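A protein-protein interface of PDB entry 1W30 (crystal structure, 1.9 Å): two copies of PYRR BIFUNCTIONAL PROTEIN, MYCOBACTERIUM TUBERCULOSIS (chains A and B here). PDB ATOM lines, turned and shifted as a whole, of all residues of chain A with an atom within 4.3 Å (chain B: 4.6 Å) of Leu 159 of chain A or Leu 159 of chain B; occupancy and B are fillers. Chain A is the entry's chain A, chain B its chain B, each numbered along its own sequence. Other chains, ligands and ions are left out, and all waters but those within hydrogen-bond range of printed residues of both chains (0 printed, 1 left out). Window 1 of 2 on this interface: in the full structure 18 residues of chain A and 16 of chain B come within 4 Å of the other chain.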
ATOM      1  N   GLY A 125     -24.930 -21.048  -1.918  1.00  0.00           N
ATOM      2  CA  GLY A 125     -24.841 -22.352  -2.528  1.00  0.00           C
ATOM      3  C   GLY A 125     -24.332 -22.264  -3.973  1.00  0.00           C
ATOM      4  O   GLY A 125     -24.062 -23.273  -4.535  1.00  0.00           O
ATOM      5  N   VAL A 128     -20.962 -23.882  -4.676  1.00  0.00           N
ATOM      6  CA  VAL A 128     -21.057 -25.339  -4.715  1.00  0.00           C
ATOM      7  C   VAL A 128     -21.665 -25.835  -6.031  1.00  0.00           C
ATOM      8  O   VAL A 128     -21.222 -26.820  -6.572  1.00  0.00           O
ATOM      9  CB  VAL A 128     -21.865 -25.844  -3.511  1.00  0.00           C
ATOM     10  CG1 VAL A 128     -22.187 -27.395  -3.611  1.00  0.00           C
ATOM     11  CG2 VAL A 128     -21.121 -25.466  -2.272  1.00  0.00           C
ATOM     12  N   ARG A 129     -22.665 -25.154  -6.542  1.00  0.00           N
ATOM     13  CA  ARG A 129     -23.254 -25.526  -7.822  1.00  0.00           C
ATOM     14  C   ARG A 129     -22.179 -25.392  -8.898  1.00  0.00           C
ATOM     15  O   ARG A 129     -21.973 -26.275  -9.720  1.00  0.00           O
ATOM     16  CB  ARG A 129     -24.450 -24.638  -8.154  1.00  0.00           C
ATOM     17  CG  ARG A 129     -25.291 -25.218  -9.289  1.00  0.00           C
ATOM     18  CD  ARG A 129     -24.796 -24.814 -10.665  1.00  0.00           C
ATOM     19  NE  ARG A 129     -25.620 -25.426 -11.707  1.00  0.00           N
ATOM     20  CZ  ARG A 129     -26.804 -24.946 -12.082  1.00  0.00           C
ATOM     21  NH1 ARG A 129     -27.299 -23.846 -11.523  1.00  0.00           N
ATOM     22  NH2 ARG A 129     -27.493 -25.554 -13.031  1.00  0.00           N
ATOM     23  N   ARG A 155     -29.639 -19.647   1.590  1.00  0.00           N
ATOM     24  CA  ARG A 155     -29.519 -20.457   0.365  1.00  0.00           C
ATOM     25  C   ARG A 155     -30.305 -19.888  -0.815  1.00  0.00           C
ATOM     26  O   ARG A 155     -31.451 -19.454  -0.674  1.00  0.00           O
ATOM     27  CB  ARG A 155     -29.990 -21.898   0.648  1.00  0.00           C
ATOM     28  CG  ARG A 155     -29.014 -22.913   0.150  1.00  0.00           C
ATOM     29  CD  ARG A 155     -28.205 -23.530   1.123  1.00  0.00           C
ATOM     30  NE  ARG A 155     -27.363 -22.533   1.701  1.00  0.00           N
ATOM     31  CZ  ARG A 155     -26.988 -22.608   2.926  1.00  0.00           C
ATOM     32  NH1 ARG A 155     -27.313 -23.698   3.637  1.00  0.00           N
ATOM     33  NH2 ARG A 155     -26.230 -21.673   3.426  1.00  0.00           N
ATOM     34  N   LEU A 157     -30.071 -21.978  -3.660  1.00  0.00           N
ATOM     35  CA  LEU A 157     -30.232 -23.261  -4.340  1.00  0.00           C
ATOM     36  C   LEU A 157     -30.507 -24.305  -3.288  1.00  0.00           C
ATOM     37  O   LEU A 157     -30.126 -24.095  -2.146  1.00  0.00           O
ATOM     38  CB  LEU A 157     -28.957 -23.601  -5.029  1.00  0.00           C
ATOM     39  CG  LEU A 157     -28.655 -22.693  -6.210  1.00  0.00           C
ATOM     40  CD1 LEU A 157     -27.316 -23.053  -6.638  1.00  0.00           C
ATOM     41  CD2 LEU A 157     -29.666 -22.759  -7.377  1.00  0.00           C
ATOM     42  N   PRO A 158     -31.173 -25.393  -3.669  1.00  0.00           N
ATOM     43  CA  PRO A 158     -31.575 -26.452  -2.727  1.00  0.00           C
ATOM     44  C   PRO A 158     -30.432 -27.363  -2.308  1.00  0.00           C
ATOM     45  O   PRO A 158     -30.508 -28.583  -2.418  1.00  0.00           O
ATOM     46  CB  PRO A 158     -32.609 -27.206  -3.511  1.00  0.00           C
ATOM     47  CG  PRO A 158     -32.278 -26.942  -4.947  1.00  0.00           C
ATOM     48  CD  PRO A 158     -31.635 -25.676  -5.033  1.00  0.00           C
ATOM     49  N   LEU A 159     -29.369 -26.741  -1.847  1.00  0.00           N
ATOM     50  CA  LEU A 159     -28.112 -27.404  -1.484  1.00  0.00           C
ATOM     51  C   LEU A 159     -27.939 -27.438   0.017  1.00  0.00           C
ATOM     52  O   LEU A 159     -28.437 -26.537   0.708  1.00  0.00           O
ATOM     53  CB  LEU A 159     -26.936 -26.645  -2.044  1.00  0.00           C
ATOM     54  CG  LEU A 159     -26.641 -26.585  -3.519  1.00  0.00           C
ATOM     55  CD1 LEU A 159     -25.484 -25.742  -3.710  1.00  0.00           C
ATOM     56  CD2 LEU A 159     -26.371 -27.936  -4.069  1.00  0.00           C
ATOM     57  N   ARG A 160     -27.246 -28.456   0.545  1.00  0.00           N
ATOM     58  CA  ARG A 160     -26.889 -28.470   1.958  1.00  0.00           C
ATOM     59  C   ARG A 160     -25.599 -29.230   2.165  1.00  0.00           C
ATOM     60  O   ARG A 160     -25.240 -30.098   1.365  1.00  0.00           O
ATOM     61  CB  ARG A 160     -27.961 -29.160   2.793  1.00  0.00           C
ATOM     62  CG  ARG A 160     -28.094 -30.607   2.402  1.00  0.00           C
ATOM     63  CD  ARG A 160     -27.817 -31.614   3.489  1.00  0.00           C
ATOM     64  NE  ARG A 160     -27.968 -32.918   2.847  1.00  0.00           N
ATOM     65  CZ  ARG A 160     -27.110 -33.448   1.981  1.00  0.00           C
ATOM     66  NH1 ARG A 160     -25.957 -32.855   1.711  1.00  0.00           N
ATOM     67  NH2 ARG A 160     -27.411 -34.612   1.414  1.00  0.00           N
ATOM     68  N   GLY B 125     -31.173 -37.384  -5.898  1.00  0.00           N
ATOM     69  CA  GLY B 125     -30.969 -35.984  -6.151  1.00  0.00           C
ATOM     70  C   GLY B 125     -30.553 -35.717  -7.578  1.00  0.00           C
ATOM     71  O   GLY B 125     -30.507 -34.587  -7.957  1.00  0.00           O
ATOM     72  N   VAL B 128     -33.121 -33.611  -9.666  1.00  0.00           N
ATOM     73  CA  VAL B 128     -33.098 -32.208  -9.287  1.00  0.00           C
ATOM     74  C   VAL B 128     -31.875 -31.474  -9.876  1.00  0.00           C
ATOM     75  O   VAL B 128     -31.956 -30.361 -10.356  1.00  0.00           O
ATOM     76  CB  VAL B 128     -33.076 -32.104  -7.771  1.00  0.00           C
ATOM     77  CG1 VAL B 128     -32.878 -30.719  -7.349  1.00  0.00           C
ATOM     78  CG2 VAL B 128     -34.387 -32.636  -7.238  1.00  0.00           C
ATOM     79  N   ARG B 129     -30.753 -32.130  -9.860  1.00  0.00           N
ATOM     80  CA  ARG B 129     -29.570 -31.570 -10.480  1.00  0.00           C
ATOM     81  C   ARG B 129     -29.793 -31.419 -11.973  1.00  0.00           C
ATOM     82  O   ARG B 129     -29.491 -30.364 -12.532  1.00  0.00           O
ATOM     83  CB  ARG B 129     -28.391 -32.419 -10.171  1.00  0.00           C
ATOM     84  CG  ARG B 129     -27.058 -31.745 -10.485  1.00  0.00           C
ATOM     85  CD  ARG B 129     -26.558 -32.059 -11.893  1.00  0.00           C
ATOM     86  NE  ARG B 129     -25.382 -31.209 -12.206  1.00  0.00           N
ATOM     87  CZ  ARG B 129     -24.117 -31.554 -12.005  1.00  0.00           C
ATOM     88  NH1 ARG B 129     -23.782 -32.754 -11.525  1.00  0.00           N
ATOM     89  NH2 ARG B 129     -23.145 -30.691 -12.317  1.00  0.00           N
ATOM     90  N   ARG B 155     -29.223 -39.945  -0.814  1.00  0.00           N
ATOM     91  CA  ARG B 155     -28.763 -38.870  -1.623  1.00  0.00           C
ATOM     92  C   ARG B 155     -27.390 -39.240  -2.221  1.00  0.00           C
ATOM     93  O   ARG B 155     -26.562 -39.793  -1.539  1.00  0.00           O
ATOM     94  CB  ARG B 155     -28.718 -37.589  -0.754  1.00  0.00           C
ATOM     95  CG  ARG B 155     -29.028 -36.408  -1.560  1.00  0.00           C
ATOM     96  CD  ARG B 155     -30.384 -35.893  -1.507  1.00  0.00           C
ATOM     97  NE  ARG B 155     -31.340 -36.913  -1.519  1.00  0.00           N
ATOM     98  CZ  ARG B 155     -32.263 -37.065  -0.595  1.00  0.00           C
ATOM     99  NH1 ARG B 155     -32.389 -36.243   0.434  1.00  0.00           N
ATOM    100  NH2 ARG B 155     -33.078 -38.052  -0.733  1.00  0.00           N
ATOM    101  N   LEU B 157     -25.937 -36.506  -4.132  1.00  0.00           N
ATOM    102  CA  LEU B 157     -25.490 -35.145  -4.364  1.00  0.00           C
ATOM    103  C   LEU B 157     -25.919 -34.357  -3.109  1.00  0.00           C
ATOM    104  O   LEU B 157     -26.806 -34.813  -2.401  1.00  0.00           O
ATOM    105  CB  LEU B 157     -26.151 -34.556  -5.605  1.00  0.00           C
ATOM    106  CG  LEU B 157     -25.865 -35.131  -6.987  1.00  0.00           C
ATOM    107  CD1 LEU B 157     -26.735 -34.416  -8.029  1.00  0.00           C
ATOM    108  CD2 LEU B 157     -24.357 -34.980  -7.275  1.00  0.00           C
ATOM    109  N   PRO B 158     -25.253 -33.248  -2.807  1.00  0.00           N
ATOM    110  CA  PRO B 158     -25.546 -32.455  -1.595  1.00  0.00           C
ATOM    111  C   PRO B 158     -26.824 -31.573  -1.753  1.00  0.00           C
ATOM    112  O   PRO B 158     -26.822 -30.370  -1.572  1.00  0.00           O
ATOM    113  CB  PRO B 158     -24.273 -31.671  -1.372  1.00  0.00           C
ATOM    114  CG  PRO B 158     -23.760 -31.437  -2.752  1.00  0.00           C
ATOM    115  CD  PRO B 158     -24.119 -32.688  -3.569  1.00  0.00           C
ATOM    116  N   LEU B 159     -27.935 -32.238  -2.012  1.00  0.00           N
ATOM    117  CA  LEU B 159     -29.233 -31.623  -2.315  1.00  0.00           C
ATOM    118  C   LEU B 159     -30.211 -32.003  -1.201  1.00  0.00           C
ATOM    119  O   LEU B 159     -30.079 -33.054  -0.550  1.00  0.00           O
ATOM    120  CB  LEU B 159     -29.734 -32.067  -3.696  1.00  0.00           C
ATOM    121  CG  LEU B 159     -28.900 -31.565  -4.916  1.00  0.00           C
ATOM    122  CD1 LEU B 159     -29.458 -31.908  -6.291  1.00  0.00           C
ATOM    123  CD2 LEU B 159     -28.695 -30.091  -4.867  1.00  0.00           C
ATOM    124  N   ARG B 160     -31.149 -31.124  -0.909  1.00  0.00           N
ATOM    125  CA  ARG B 160     -32.239 -31.448   0.007  1.00  0.00           C
ATOM    126  C   ARG B 160     -33.458 -30.632  -0.389  1.00  0.00           C
ATOM    127  O   ARG B 160     -33.366 -29.608  -1.052  1.00  0.00           O
ATOM    128  CB  ARG B 160     -31.906 -31.140   1.449  1.00  0.00           C
ATOM    129  CG  ARG B 160     -31.350 -29.728   1.686  1.00  0.00           C
ATOM    130  CD  ARG B 160     -32.342 -28.660   2.066  1.00  0.00           C
ATOM    131  NE  ARG B 160     -32.403 -28.309   3.493  1.00  0.00           N
ATOM    132  CZ  ARG B 160     -33.301 -27.436   4.007  1.00  0.00           C
ATOM    133  NH1 ARG B 160     -34.183 -26.825   3.228  1.00  0.00           N
ATOM    134  NH2 ARG B 160     -33.312 -27.162   5.305  1.00  0.00           N
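The backbone NH (N) of Arg 160 of chain A lies within hydrogen-bond range of the backbone carbonyl oxygen (O) of Pro 158 of chain B (2.9 Å).
The backbone NH (N) of Arg 160 of chain B sits at hydrogen-bond distance from the backbone carbonyl oxygen (O) of Pro 158 of chain A (3.0 Å).
Among the printed residues, merely in contact across the chains: Leu 159 of chain A with Pro 158 of chain B (3.2 Å), Leu 159 of chain A with Leu 159 of chain B (3.3 Å), Pro 158 of chain A with Leu 159 of chain B (3.3 Å), Arg 160 of chain A with Arg 160 of chain B (3.4 Å), Arg 160 of chain A with Leu 159 of chain B (3.7 Å), Arg 160 of chain A with Arg 155 of chain B (3.8 Å) and Arg 160 of chain A with Leu 157 of chain B (3.9 Å).
Of the printed residues of chain B, Leu 159 of chain A touches Pro 158 and Leu 159.
Of chain A, only Pro 158, Leu 159 and Arg 160 come within 4 Å of Leu 159 of chain B.
Of the printed residues of chain A, Arg 155 of chain B touches Arg 160 (3.8 Å).
Of the printed residues of chain A, Arg 160 of chain B touches Pro 158 (3.0 Å) and Arg 160 (3.4 Å).
Of the printed residues of chain B, Pro 158 of chain A touches Leu 159 (3.3 Å) and Arg 160 (3.0 Å).
Of the printed residues of chain B, Arg 160 of chain A touches Arg 155 (3.8 Å), Leu 157 (3.9 Å), Pro 158 (2.9 Å), Leu 159 (3.7 Å) and Arg 160 (3.4 Å).
Of the printed residues of chain A, Pro 158 of chain B touches Leu 159 and Arg 160.
Val 128 of chain A touches none of the printed residues of chain B.
The nearest residue of chain B that does not touch Leu 159 of chain A is Arg 160 of chain B (4.4 Å).
The nearest printed residue of chain A that does not touch Leu 159 of chain B is Leu 157 of chain A (6.3 Å).
Of the 8 printed residues of chain A, 3 touch a printed residue of chain B.
Printed residues of chain A that touch a printed residue of chain B: Pro 158, Leu 159 and Arg 160.
Of the 8 printed residues of chain B, 5 touch a printed residue of chain A.
Printed residues of chain B that touch a printed residue of chain A: Arg 155, Leu 157, Pro 158, Leu 159 and Arg 160.
Hydrophobic or aromatic side chains of chain B that line the printed part of chain A: Pro 158 and Leu 159.
Pro 158 of chain A touches Leu 159 of chain B, and with the chains exchanged Leu 159 of chain A touches Pro 158 of chain B.
Leu 159 of chain B touches its own counterpart, Leu 159 of chain A.
Arg 160 of chain A touches Leu 157 of chain B, but with the chains exchanged Leu 157 of chain A does not touch Arg 160 of chain B (6.4 Å).
Arg 160 of chain A touches its own counterpart, Arg 160 of chain B.
Of the 9 pairs that touch across the chains among the printed residues, 6 have their exchanged pair printed and touching as well.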
